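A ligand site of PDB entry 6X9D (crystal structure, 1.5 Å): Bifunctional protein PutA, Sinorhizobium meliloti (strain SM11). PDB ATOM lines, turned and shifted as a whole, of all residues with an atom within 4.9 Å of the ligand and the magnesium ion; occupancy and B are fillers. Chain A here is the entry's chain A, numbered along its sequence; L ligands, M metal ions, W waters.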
ATOM      1  N   ILE A 705      13.405  22.997  10.740  1.00  0.00           N
ATOM      2  CA  ILE A 705      12.670  24.192  11.102  1.00  0.00           C
ATOM      3  C   ILE A 705      13.487  24.913  12.170  1.00  0.00           C
ATOM      4  O   ILE A 705      13.852  24.300  13.183  1.00  0.00           O
ATOM      5  CB  ILE A 705      11.259  23.827  11.619  1.00  0.00           C
ATOM      6  CG1 ILE A 705      10.413  23.255  10.479  1.00  0.00           C
ATOM      7  CG2 ILE A 705      10.573  25.028  12.215  1.00  0.00           C
ATOM      8  CD1 ILE A 705       9.145  22.586  10.980  1.00  0.00           C
ATOM      9  N   SER A 706      13.780  26.179  11.932  1.00  0.00           N
ATOM     10  CA  SER A 706      14.748  26.898  12.744  1.00  0.00           C
ATOM     11  C   SER A 706      14.165  28.199  13.274  1.00  0.00           C
ATOM     12  O   SER A 706      13.190  28.725  12.737  1.00  0.00           O
ATOM     13  CB  SER A 706      16.034  27.176  11.950  1.00  0.00           C
ATOM     14  OG  SER A 706      15.750  27.806  10.702  1.00  0.00           O
ATOM     15  N   PRO A 707      14.752  28.740  14.346  1.00  0.00           N
ATOM     16  CA  PRO A 707      14.255  29.976  14.950  1.00  0.00           C
ATOM     17  C   PRO A 707      14.912  31.205  14.339  1.00  0.00           C
ATOM     18  O   PRO A 707      15.886  31.127  13.600  1.00  0.00           O
ATOM     19  CB  PRO A 707      14.660  29.814  16.410  1.00  0.00           C
ATOM     20  CG  PRO A 707      15.971  29.116  16.318  1.00  0.00           C
ATOM     21  CD  PRO A 707      15.790  28.113  15.183  1.00  0.00           C
ATOM     22  N   TRP A 708      14.353  32.371  14.662  1.00  0.00           N
ATOM     23  CA  TRP A 708      14.890  33.614  14.112  1.00  0.00           C
ATOM     24  C   TRP A 708      16.162  34.062  14.833  1.00  0.00           C
ATOM     25  O   TRP A 708      16.941  34.819  14.237  1.00  0.00           O
ATOM     26  CB  TRP A 708      13.839  34.732  14.181  1.00  0.00           C
ATOM     27  CG  TRP A 708      13.665  35.241  15.567  1.00  0.00           C
ATOM     28  CD1 TRP A 708      12.712  34.843  16.464  1.00  0.00           C
ATOM     29  CD2 TRP A 708      14.501  36.189  16.251  1.00  0.00           C
ATOM     30  NE1 TRP A 708      12.910  35.495  17.661  1.00  0.00           N
ATOM     31  CE2 TRP A 708      14.000  36.326  17.547  1.00  0.00           C
ATOM     32  CE3 TRP A 708      15.616  36.955  15.877  1.00  0.00           C
ATOM     33  CZ2 TRP A 708      14.570  37.184  18.484  1.00  0.00           C
ATOM     34  CZ3 TRP A 708      16.190  37.793  16.800  1.00  0.00           C
ATOM     35  CH2 TRP A 708      15.665  37.901  18.090  1.00  0.00           C
ATOM     36  N   ASN A 709      16.388  33.623  16.071  1.00  0.00           N
ATOM     37  CA  ASN A 709      17.370  34.305  16.919  1.00  0.00           C
ATOM     38  C   ASN A 709      18.794  33.819  16.701  1.00  0.00           C
ATOM     39  O   ASN A 709      19.723  34.525  17.096  1.00  0.00           O
ATOM     40  CB  ASN A 709      16.983  34.159  18.391  1.00  0.00           C
ATOM     41  CG  ASN A 709      17.060  32.734  18.887  1.00  0.00           C
ATOM     42  OD1 ASN A 709      16.578  31.807  18.244  1.00  0.00           O
ATOM     43  ND2 ASN A 709      17.656  32.560  20.058  1.00  0.00           N
ATOM     44  N   PHE A 710      18.986  32.661  16.086  1.00  0.00           N
ATOM     45  CA  PHE A 710      20.284  32.257  15.563  1.00  0.00           C
ATOM     46  C   PHE A 710      20.060  31.903  14.109  1.00  0.00           C
ATOM     47  O   PHE A 710      20.054  30.734  13.727  1.00  0.00           O
ATOM     48  CB  PHE A 710      20.904  31.109  16.363  1.00  0.00           C
ATOM     49  CG  PHE A 710      21.175  31.468  17.799  1.00  0.00           C
ATOM     50  CD1 PHE A 710      22.205  32.343  18.120  1.00  0.00           C
ATOM     51  CD2 PHE A 710      20.371  30.981  18.806  1.00  0.00           C
ATOM     52  CE1 PHE A 710      22.451  32.699  19.451  1.00  0.00           C
ATOM     53  CE2 PHE A 710      20.616  31.333  20.127  1.00  0.00           C
ATOM     54  CZ  PHE A 710      21.641  32.196  20.444  1.00  0.00           C
ATOM     55  N   ILE A 714      22.085  28.090  13.926  1.00  0.00           N
ATOM     56  CA  ILE A 714      21.218  26.938  14.166  1.00  0.00           C
ATOM     57  C   ILE A 714      20.590  26.461  12.863  1.00  0.00           C
ATOM     58  O   ILE A 714      20.427  25.258  12.633  1.00  0.00           O
ATOM     59  CB  ILE A 714      20.154  27.275  15.229  1.00  0.00           C
ATOM     60  CG1 ILE A 714      20.846  27.331  16.597  1.00  0.00           C
ATOM     61  CG2 ILE A 714      19.024  26.232  15.264  1.00  0.00           C
ATOM     62  CD1 ILE A 714      19.904  27.537  17.758  1.00  0.00           C
ATOM     63  N   LYS A 732      13.185  25.180   6.397  1.00  0.00           N
ATOM     64  CA  LYS A 732      12.134  26.174   6.607  1.00  0.00           C
ATOM     65  C   LYS A 732      12.646  27.168   7.645  1.00  0.00           C
ATOM     66  O   LYS A 732      12.527  26.937   8.851  1.00  0.00           O
ATOM     67  CB  LYS A 732      10.829  25.513   7.065  1.00  0.00           C
ATOM     68  CG  LYS A 732       9.569  26.173   6.577  1.00  0.00           C
ATOM     69  CD  LYS A 732       9.429  27.628   7.059  1.00  0.00           C
ATOM     70  CE  LYS A 732       9.300  27.710   8.580  1.00  0.00           C
ATOM     71  NZ  LYS A 732       9.103  29.104   9.029  1.00  0.00           N
ATOM     72  N   PRO A 733      13.222  28.295   7.218  1.00  0.00           N
ATOM     73  CA  PRO A 733      13.725  29.282   8.183  1.00  0.00           C
ATOM     74  C   PRO A 733      12.589  30.075   8.794  1.00  0.00           C
ATOM     75  O   PRO A 733      11.480  30.162   8.241  1.00  0.00           O
ATOM     76  CB  PRO A 733      14.611  30.188   7.325  1.00  0.00           C
ATOM     77  CG  PRO A 733      13.931  30.164   5.986  1.00  0.00           C
ATOM     78  CD  PRO A 733      13.378  28.754   5.821  1.00  0.00           C
ATOM     79  N   ALA A 734      12.886  30.668   9.940  1.00  0.00           N
ATOM     80  CA  ALA A 734      11.922  31.516  10.609  1.00  0.00           C
ATOM     81  C   ALA A 734      11.460  32.624   9.655  1.00  0.00           C
ATOM     82  O   ALA A 734      12.247  33.135   8.858  1.00  0.00           O
ATOM     83  CB  ALA A 734      12.533  32.123  11.868  1.00  0.00           C
ATOM     84  N   GLU A 735      10.188  32.987   9.767  1.00  0.00           N
ATOM     85  CA  GLU A 735       9.668  34.019   8.874  1.00  0.00           C
ATOM     86  C   GLU A 735      10.364  35.362   9.063  1.00  0.00           C
ATOM     87  O   GLU A 735      10.415  36.167   8.131  1.00  0.00           O
ATOM     88  CB  GLU A 735       8.160  34.177   9.056  1.00  0.00           C
ATOM     89  CG  GLU A 735       7.680  34.390  10.481  1.00  0.00           C
ATOM     90  CD  GLU A 735       7.421  33.099  11.252  1.00  0.00           C
ATOM     91  OE1 GLU A 735       8.022  32.052  10.916  1.00  0.00           O
ATOM     92  OE2 GLU A 735       6.616  33.127  12.201  1.00  0.00           O
ATOM     93  N   GLU A 736      10.936  35.611  10.240  1.00  0.00           N
ATOM     94  CA  GLU A 736      11.564  36.907  10.490  1.00  0.00           C
ATOM     95  C   GLU A 736      12.907  37.053   9.779  1.00  0.00           C
ATOM     96  O   GLU A 736      13.317  38.172   9.472  1.00  0.00           O
ATOM     97  CB  GLU A 736      11.756  37.120  11.997  1.00  0.00           C
ATOM     98  CG  GLU A 736      10.454  37.132  12.777  1.00  0.00           C
ATOM     99  CD  GLU A 736      10.051  35.772  13.341  1.00  0.00           C
ATOM    100  OE1 GLU A 736       9.303  35.768  14.353  1.00  0.00           O
ATOM    101  OE2 GLU A 736      10.480  34.722  12.806  1.00  0.00           O
ATOM    102  N   GLY A 763       8.891  31.157   4.698  1.00  0.00           N
ATOM    103  CA  GLY A 763       7.504  31.354   5.080  1.00  0.00           C
ATOM    104  C   GLY A 763       7.327  31.166   6.569  1.00  0.00           C
ATOM    105  O   GLY A 763       8.297  31.020   7.316  1.00  0.00           O
ATOM    106  N   ASP A 764       6.070  31.164   6.990  1.00  0.00           N
ATOM    107  CA  ASP A 764       5.722  31.175   8.401  1.00  0.00           C
ATOM    108  C   ASP A 764       5.420  29.757   8.891  1.00  0.00           C
ATOM    109  O   ASP A 764       5.831  28.753   8.284  1.00  0.00           O
ATOM    110  CB  ASP A 764       4.544  32.130   8.630  1.00  0.00           C
ATOM    111  CG  ASP A 764       3.282  31.748   7.858  1.00  0.00           C
ATOM    112  OD1 ASP A 764       3.090  30.563   7.536  1.00  0.00           O
ATOM    113  OD2 ASP A 764       2.489  32.661   7.550  1.00  0.00           O
ATOM    114  N   GLY A 765       4.709  29.658  10.017  1.00  0.00           N
ATOM    115  CA  GLY A 765       4.517  28.373  10.668  1.00  0.00           C
ATOM    116  C   GLY A 765       3.704  27.383   9.869  1.00  0.00           C
ATOM    117  O   GLY A 765       3.846  26.181  10.065  1.00  0.00           O
ATOM    118  N   GLY A 768       5.976  25.534   7.774  1.00  0.00           N
ATOM    119  CA  GLY A 768       6.547  24.511   8.635  1.00  0.00           C
ATOM    120  C   GLY A 768       5.591  23.350   8.844  1.00  0.00           C
ATOM    121  O   GLY A 768       5.981  22.185   8.735  1.00  0.00           O
ATOM    122  N   ALA A 769       4.323  23.652   9.134  1.00  0.00           N
ATOM    123  CA  ALA A 769       3.368  22.587   9.444  1.00  0.00           C
ATOM    124  C   ALA A 769       3.069  21.747   8.208  1.00  0.00           C
ATOM    125  O   ALA A 769       2.894  20.525   8.305  1.00  0.00           O
ATOM    126  CB  ALA A 769       2.081  23.175  10.008  1.00  0.00           C
ATOM    127  N   VAL A 772       5.928  19.333   7.891  1.00  0.00           N
ATOM    128  CA  VAL A 772       5.860  18.301   8.912  1.00  0.00           C
ATOM    129  C   VAL A 772       4.806  17.262   8.554  1.00  0.00           C
ATOM    130  O   VAL A 772       5.036  16.051   8.690  1.00  0.00           O
ATOM    131  CB  VAL A 772       5.612  18.939  10.294  1.00  0.00           C
ATOM    132  CG1 VAL A 772       5.244  17.874  11.329  1.00  0.00           C
ATOM    133  CG2 VAL A 772       6.851  19.692  10.767  1.00  0.00           C
ATOM    134  N   PHE A 782      13.660  20.404  14.893  1.00  0.00           N
ATOM    135  CA  PHE A 782      12.991  21.633  15.289  1.00  0.00           C
ATOM    136  C   PHE A 782      13.773  22.307  16.403  1.00  0.00           C
ATOM    137  O   PHE A 782      14.120  21.674  17.404  1.00  0.00           O
ATOM    138  CB  PHE A 782      11.568  21.366  15.798  1.00  0.00           C
ATOM    139  CG  PHE A 782      10.894  22.584  16.341  1.00  0.00           C
ATOM    140  CD1 PHE A 782      10.311  23.505  15.481  1.00  0.00           C
ATOM    141  CD2 PHE A 782      10.884  22.837  17.710  1.00  0.00           C
ATOM    142  CE1 PHE A 782       9.705  24.643  15.975  1.00  0.00           C
ATOM    143  CE2 PHE A 782      10.274  23.967  18.208  1.00  0.00           C
ATOM    144  CZ  PHE A 782       9.687  24.876  17.343  1.00  0.00           C
ATOM    145  N   THR A 783      14.019  23.600  16.224  1.00  0.00           N
ATOM    146  CA  THR A 783      14.497  24.446  17.296  1.00  0.00           C
ATOM    147  C   THR A 783      13.574  25.657  17.355  1.00  0.00           C
ATOM    148  O   THR A 783      13.313  26.279  16.316  1.00  0.00           O
ATOM    149  CB  THR A 783      15.972  24.836  17.068  1.00  0.00           C
ATOM    150  OG1 THR A 783      16.764  23.648  17.003  1.00  0.00           O
ATOM    151  CG2 THR A 783      16.473  25.673  18.219  1.00  0.00           C
ATOM    152  N   GLY A 784      13.034  25.938  18.539  1.00  0.00           N
ATOM    153  CA  GLY A 784      12.045  26.987  18.675  1.00  0.00           C
ATOM    154  C   GLY A 784      11.346  26.879  20.022  1.00  0.00           C
ATOM    155  O   GLY A 784      11.873  26.271  20.949  1.00  0.00           O
ATOM    156  N   SER A 785      10.157  27.452  20.099  1.00  0.00           N
ATOM    157  CA  SER A 785       9.439  27.440  21.374  1.00  0.00           C
ATOM    158  C   SER A 785       8.880  26.057  21.713  1.00  0.00           C
ATOM    159  O   SER A 785       8.563  25.239  20.830  1.00  0.00           O
ATOM    160  CB  SER A 785       8.293  28.448  21.347  1.00  0.00           C
ATOM    161  OG  SER A 785       7.319  28.070  20.411  1.00  0.00           O
ATOM    162  N   THR A 786       8.741  25.796  23.011  1.00  0.00           N
ATOM    163  CA  THR A 786       8.158  24.534  23.476  1.00  0.00           C
ATOM    164  C   THR A 786       6.723  24.357  22.984  1.00  0.00           C
ATOM    165  O   THR A 786       6.318  23.238  22.667  1.00  0.00           O
ATOM    166  CB  THR A 786       8.213  24.459  25.001  1.00  0.00           C
ATOM    167  OG1 THR A 786       9.555  24.688  25.437  1.00  0.00           O
ATOM    168  CG2 THR A 786       7.743  23.083  25.491  1.00  0.00           C
ATOM    169  N   VAL A 788       5.342  25.374  20.166  1.00  0.00           N
ATOM    170  CA  VAL A 788       5.289  24.944  18.770  1.00  0.00           C
ATOM    171  C   VAL A 788       5.811  23.525  18.637  1.00  0.00           C
ATOM    172  O   VAL A 788       5.231  22.708  17.902  1.00  0.00           O
ATOM    173  CB  VAL A 788       6.071  25.935  17.887  1.00  0.00           C
ATOM    174  CG1 VAL A 788       6.276  25.370  16.489  1.00  0.00           C
ATOM    175  CG2 VAL A 788       5.319  27.265  17.811  1.00  0.00           C
ATOM    176  N   LEU A 791       3.059  21.236  19.229  1.00  0.00           N
ATOM    177  CA  LEU A 791       2.160  21.071  18.084  1.00  0.00           C
ATOM    178  C   LEU A 791       2.751  20.126  17.049  1.00  0.00           C
ATOM    179  O   LEU A 791       2.033  19.296  16.477  1.00  0.00           O
ATOM    180  CB  LEU A 791       1.849  22.433  17.454  1.00  0.00           C
ATOM    181  CG  LEU A 791       1.027  23.415  18.289  1.00  0.00           C
ATOM    182  CD1 LEU A 791       1.053  24.798  17.658  1.00  0.00           C
ATOM    183  CD2 LEU A 791      -0.402  22.913  18.429  1.00  0.00           C
ATOM    184  N   ILE A 792       4.058  20.223  16.801  1.00  0.00           N
ATOM    185  CA  ILE A 792       4.711  19.293  15.884  1.00  0.00           C
ATOM    186  C   ILE A 792       4.663  17.866  16.428  1.00  0.00           C
ATOM    187  O   ILE A 792       4.378  16.919  15.685  1.00  0.00           O
ATOM    188  CB  ILE A 792       6.156  19.753  15.597  1.00  0.00           C
ATOM    189  CG1 ILE A 792       6.154  21.037  14.781  1.00  0.00           C
ATOM    190  CG2 ILE A 792       6.968  18.646  14.892  1.00  0.00           C
ATOM    191  CD1 ILE A 792       7.477  21.747  14.770  1.00  0.00           C
ATOM    192  N   GLU A 812      14.437  21.103  20.210  1.00  0.00           N
ATOM    193  CA  GLU A 812      15.259  21.838  21.161  1.00  0.00           C
ATOM    194  C   GLU A 812      14.547  23.153  21.470  1.00  0.00           C
ATOM    195  O   GLU A 812      14.298  23.950  20.552  1.00  0.00           O
ATOM    196  CB  GLU A 812      16.659  22.044  20.605  1.00  0.00           C
ATOM    197  CG  GLU A 812      17.347  20.697  20.280  1.00  0.00           C
ATOM    198  CD  GLU A 812      17.514  19.820  21.527  1.00  0.00           C
ATOM    199  OE1 GLU A 812      18.470  20.046  22.279  1.00  0.00           O
ATOM    200  OE2 GLU A 812      16.672  18.921  21.742  1.00  0.00           O
ATOM    201  N   THR A 813      14.184  23.351  22.726  1.00  0.00           N
ATOM    202  CA  THR A 813      13.173  24.351  23.016  1.00  0.00           C
ATOM    203  C   THR A 813      13.626  25.340  24.084  1.00  0.00           C
ATOM    204  O   THR A 813      14.835  25.584  24.221  1.00  0.00           O
ATOM    205  CB  THR A 813      11.855  23.643  23.386  1.00  0.00           C
ATOM    206  OG1 THR A 813      12.100  22.561  24.308  1.00  0.00           O
ATOM    207  CG2 THR A 813      11.243  23.035  22.127  1.00  0.00           C
ATOM    208  N   GLY A 814      12.692  25.942  24.822  1.00  0.00           N
ATOM    209  CA  GLY A 814      13.024  27.109  25.618  1.00  0.00           C
ATOM    210  C   GLY A 814      13.711  26.790  26.929  1.00  0.00           C
ATOM    211  O   GLY A 814      13.857  25.634  27.324  1.00  0.00           O
ATOM    212  N   GLY A 815      14.128  27.854  27.619  1.00  0.00           N
ATOM    213  CA  GLY A 815      14.774  27.715  28.912  1.00  0.00           C
ATOM    214  C   GLY A 815      14.220  28.735  29.888  1.00  0.00           C
ATOM    215  O   GLY A 815      13.566  29.704  29.508  1.00  0.00           O
ATOM    216  N   CYS A 846      18.368  31.562  23.563  1.00  0.00           N
ATOM    217  CA  CYS A 846      17.693  30.554  24.366  1.00  0.00           C
ATOM    218  C   CYS A 846      18.446  30.285  25.670  1.00  0.00           C
ATOM    219  O   CYS A 846      17.829  29.899  26.669  1.00  0.00           O
ATOM    220  CB  CYS A 846      17.538  29.267  23.569  1.00  0.00           C
ATOM    221  SG  CYS A 846      19.088  28.698  22.827  1.00  0.00           S
ATOM    222  N   GLU A 942       8.811  31.329  29.865  1.00  0.00           N
ATOM    223  CA  GLU A 942      10.008  31.977  29.326  1.00  0.00           C
ATOM    224  C   GLU A 942       9.617  33.309  28.706  1.00  0.00           C
ATOM    225  O   GLU A 942       8.698  33.383  27.887  1.00  0.00           O
ATOM    226  CB  GLU A 942      10.665  31.058  28.284  1.00  0.00           C
ATOM    227  CG  GLU A 942      11.825  31.677  27.499  1.00  0.00           C
ATOM    228  CD  GLU A 942      12.193  30.863  26.267  1.00  0.00           C
ATOM    229  OE1 GLU A 942      13.366  30.445  26.146  1.00  0.00           O
ATOM    230  OE2 GLU A 942      11.304  30.644  25.395  1.00  0.00           O
ATOM    231  N   PHE A 944      11.071  36.029  26.437  1.00  0.00           N
ATOM    232  CA  PHE A 944      12.198  35.989  25.502  1.00  0.00           C
ATOM    233  C   PHE A 944      12.624  37.414  25.148  1.00  0.00           C
ATOM    234  O   PHE A 944      12.434  37.908  24.036  1.00  0.00           O
ATOM    235  CB  PHE A 944      11.821  35.192  24.255  1.00  0.00           C
ATOM    236  CG  PHE A 944      13.000  34.585  23.570  1.00  0.00           C
ATOM    237  CD1 PHE A 944      13.739  33.577  24.177  1.00  0.00           C
ATOM    238  CD2 PHE A 944      13.392  35.009  22.305  1.00  0.00           C
ATOM    239  CE1 PHE A 944      14.839  33.024  23.553  1.00  0.00           C
ATOM    240  CE2 PHE A 944      14.491  34.452  21.672  1.00  0.00           C
ATOM    241  CZ  PHE A 944      15.215  33.464  22.305  1.00  0.00           C
ATOM    242  N   LEU A 972      17.880  24.009  30.558  1.00  0.00           N
ATOM    243  CA  LEU A 972      18.748  24.319  29.423  1.00  0.00           C
ATOM    244  C   LEU A 972      20.117  24.772  29.924  1.00  0.00           C
ATOM    245  O   LEU A 972      21.015  23.942  30.054  1.00  0.00           O
ATOM    246  CB  LEU A 972      18.084  25.374  28.537  1.00  0.00           C
ATOM    247  CG  LEU A 972      18.730  25.660  27.184  1.00  0.00           C
ATOM    248  CD1 LEU A 972      19.072  24.372  26.444  1.00  0.00           C
ATOM    249  CD2 LEU A 972      17.765  26.510  26.352  1.00  0.00           C
ATOM    250  N   PHE A1012      25.581  21.510  23.106  1.00  0.00           N
ATOM    251  CA  PHE A1012      24.512  22.363  23.608  1.00  0.00           C
ATOM    252  C   PHE A1012      23.162  21.675  23.513  1.00  0.00           C
ATOM    253  O   PHE A1012      22.777  21.194  22.438  1.00  0.00           O
ATOM    254  CB  PHE A1012      24.453  23.682  22.859  1.00  0.00           C
ATOM    255  CG  PHE A1012      23.469  24.645  23.447  1.00  0.00           C
ATOM    256  CD1 PHE A1012      23.792  25.349  24.598  1.00  0.00           C
ATOM    257  CD2 PHE A1012      22.219  24.829  22.857  1.00  0.00           C
ATOM    258  CE1 PHE A1012      22.891  26.224  25.160  1.00  0.00           C
ATOM    259  CE2 PHE A1012      21.313  25.716  23.414  1.00  0.00           C
ATOM    260  CZ  PHE A1012      21.649  26.424  24.561  1.00  0.00           C
ATOM    261  N   SER A1018      13.043  21.863  27.910  1.00  0.00           N
ATOM    262  CA  SER A1018      14.074  22.509  27.105  1.00  0.00           C
ATOM    263  C   SER A1018      14.573  21.659  25.952  1.00  0.00           C
ATOM    264  O   SER A1018      15.295  22.187  25.100  1.00  0.00           O
ATOM    265  CB  SER A1018      15.284  22.888  27.972  1.00  0.00           C
ATOM    266  OG  SER A1018      14.913  23.829  28.963  1.00  0.00           O
HETATM  267  P1  LIG L   1       9.028  29.723  17.228  1.00  0.00           P
HETATM  268  O1  LIG L   1       8.478  28.566  17.994  1.00  0.00           O
HETATM  269  O2  LIG L   1       8.066  30.868  17.287  1.00  0.00           O
HETATM  270  O3  LIG L   1       9.304  29.314  15.646  1.00  0.00           O
HETATM  271  C1  LIG L   1      10.432  28.521  15.276  1.00  0.00           C
HETATM  272  C2  LIG L   1      10.115  27.981  13.847  1.00  0.00           C
HETATM  273  O4  LIG L   1       8.757  27.127  13.923  1.00  0.00           O
HETATM  274  C3  LIG L   1       9.908  28.933  12.966  1.00  0.00           C
HETATM  275  O5  LIG L   1      10.652  28.603  11.705  1.00  0.00           O
HETATM  276  C4  LIG L   1       8.379  28.963  12.712  1.00  0.00           C
HETATM  277  O6  LIG L   1       8.105  29.439  11.454  1.00  0.00           O
HETATM  278  C5  LIG L   1       7.986  27.508  12.911  1.00  0.00           C
HETATM  279  N1  LIG L   1       6.611  27.390  13.351  1.00  0.00           N
HETATM  280  C6  LIG L   1       5.741  28.150  14.003  1.00  0.00           C
HETATM  281  N2  LIG L   1       4.609  27.420  14.110  1.00  0.00           N
HETATM  282  C7  LIG L   1       4.810  26.213  13.526  1.00  0.00           C
HETATM  283  C8  LIG L   1       3.972  25.105  13.361  1.00  0.00           C
HETATM  284  N3  LIG L   1       2.587  25.103  13.882  1.00  0.00           N
HETATM  285  N4  LIG L   1       4.428  24.024  12.738  1.00  0.00           N
HETATM  286  C9  LIG L   1       5.714  24.003  12.248  1.00  0.00           C
HETATM  287  N5  LIG L   1       6.524  25.070  12.401  1.00  0.00           N
HETATM  288  C10 LIG L   1       6.057  26.182  13.055  1.00  0.00           C
HETATM  289  O7  LIG L   1      10.457  30.149  17.931  1.00  0.00           O
HETATM  290  P2  LIG L   1      11.402  31.496  17.621  1.00  0.00           P
HETATM  291  O8  LIG L   1      10.610  32.746  18.042  1.00  0.00           O
HETATM  292  O9  LIG L   1      11.848  31.556  16.179  1.00  0.00           O
HETATM  293  O10 LIG L   1      12.683  31.358  18.637  1.00  0.00           O
HETATM  294  C11 LIG L   1      12.431  31.608  20.012  1.00  0.00           C
HETATM  295  C12 LIG L   1      12.282  30.330  20.841  1.00  0.00           C
HETATM  296  O11 LIG L   1      13.353  29.252  20.326  1.00  0.00           O
HETATM  297  C13 LIG L   1      12.544  30.540  22.134  1.00  0.00           C
HETATM  298  O12 LIG L   1      11.530  29.791  22.993  1.00  0.00           O
HETATM  299  C14 LIG L   1      13.922  29.981  22.369  1.00  0.00           C
HETATM  300  O13 LIG L   1      14.134  29.577  23.691  1.00  0.00           O
HETATM  301  C15 LIG L   1      13.889  28.764  21.387  1.00  0.00           C
HETATM  302  N6  LIG L   1      15.293  28.370  21.089  1.00  0.00           N
HETATM  303  C16 LIG L   1      15.811  27.184  21.588  1.00  0.00           C
HETATM  304  C17 LIG L   1      17.123  26.879  21.284  1.00  0.00           C
HETATM  305  C18 LIG L   1      17.790  25.561  21.802  1.00  0.00           C
HETATM  306  O14 LIG L   1      18.819  25.200  21.333  1.00  0.00           O
HETATM  307  N7  LIG L   1      17.136  24.805  22.898  1.00  0.00           N
HETATM  308  C19 LIG L   1      17.862  27.704  20.466  1.00  0.00           C
HETATM  309  C20 LIG L   1      17.352  28.893  20.008  1.00  0.00           C
HETATM  310  C21 LIG L   1      16.041  29.203  20.322  1.00  0.00           C
HETATM  311 MG    MG M   1       7.382  32.650  16.340  1.00  0.00          MG
HETATM  312  O   HOH W   1       8.966  33.843  16.510  1.00  0.00           O
HETATM  313  O   HOH W   2       6.460  32.919  18.151  1.00  0.00           O
HETATM  314  O   HOH W   3      17.759  22.066  24.078  1.00  0.00           O
HETATM  315  O   HOH W   4       7.656  31.820  14.283  1.00  0.00           O
HETATM  316  O   HOH W   5      20.395  23.555  19.881  1.00  0.00           O
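The side-chain carboxylate of Glu 735 lies within salt-bridge range of the side-chain amino group of Lys 732, at 3.7 Å. The backbone carbonyl oxygen (O) of Asp 764 is in hydrogen-bond range of the side-chain amino group (NZ) of Lys 732, at 3.4 Å. O of Ser 706 is in hydrogen-bond range of N of Ala 734 (3.4 Å). N of Thr 813 is in hydrogen-bond range of O of Ser 1018 (2.9 Å). The backbone carbonyl oxygen (O) of Glu 812 sits at hydrogen-bond distance from the backbone NH (N) of Gly 784. O of Gly 814 sits at hydrogen-bond distance from OG of Ser 1018 (2.7 Å). OG1 of Thr 786 is in hydrogen-bond range of N of Gly 814 (3.4 Å). The side-chain hydroxyl (OG) of Ser 1018 sits at hydrogen-bond distance from the backbone NH (N) of Leu 972, 3.4 Å away.
The magnesium ion is bound by water W1 (2.0 Å), water W2 (2.0 Å), an oxygen (O2) of the ligand (2.1 Å) and water W4 (2.2 Å).
No residue comes within 4 Å of the magnesium ion.
Water W4 bridges OE2 of Glu 735 and O3 of the ligand. Water W1 lies within hydrogen-bond range of O8 of the ligand (2.5 Å) and OE1 of Glu 736 (2.9 Å). Water W3 lies within hydrogen-bond range of O of Ser 1018, OE1 of Glu 812 and N7 of the ligand.
The backbone carbonyl oxygen (O) of Gly 765 sits close to a nitrogen (N4) of the ligand, at 3.5 Å. The backbone carbonyl oxygen of Gly 784 lies close to an oxygen (O11) of the ligand (3.4 Å). Merely in contact with the ligand: Ile 705 (3.3 Å), Pro 707 (3.1 Å), Asn 709 (3.4 Å), Phe 710 (3.9 Å), Ile 714 (3.4 Å), Pro 733 (3.8 Å), Ala 734 (3.4 Å), Asp 764 (3.7 Å), Gly 768 (3.5 Å), Ala 769 (3.4 Å), Phe 782 (3.4 Å), Thr 783 (3.3 Å), Val 788 (3.4 Å), Ile 792 (3.8 Å), Glu 812 (3.4 Å), Gly 814 (3.3 Å), Cys 846 (2.8 Å), Phe 944 (3.4 Å), Leu 972 (3.9 Å), Phe 1012 (3.3 Å) and Ser 1018 (3.9 Å). Hydrophobic or aromatic side chains that line the ligand: Ile 705, Pro 707, Trp 708, Phe 710, Ile 714, Ala 734, Ala 769, Phe 782, Val 788, Ile 792, Phe 944, Leu 972 and Phe 1012.
An oxygen (O12) of the ligand is in hydrogen-bond range of the side-chain carboxylate (OE2) of Glu 942 (2.6 Å). NZ of Lys 732 sits at hydrogen-bond distance from O6 of the ligand, at 2.6 Å. OE1 of Glu 735 sits at hydrogen-bond distance from O6 of the ligand, 2.7 Å away. N of Ser 785 lies within hydrogen-bond range of O1 of the ligand (2.9 Å). O1 of the ligand lies within hydrogen-bond range of OG of Ser 785. O of Ser 706 lies within hydrogen-bond range of O5 of the ligand, 2.7 Å away. The backbone carbonyl oxygen of Thr 813 is in hydrogen-bond range of a nitrogen (N7) of the ligand (2.8 Å). An oxygen (O9) of the ligand lies within hydrogen-bond range of the backbone NH of Trp 708 (3.0 Å).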
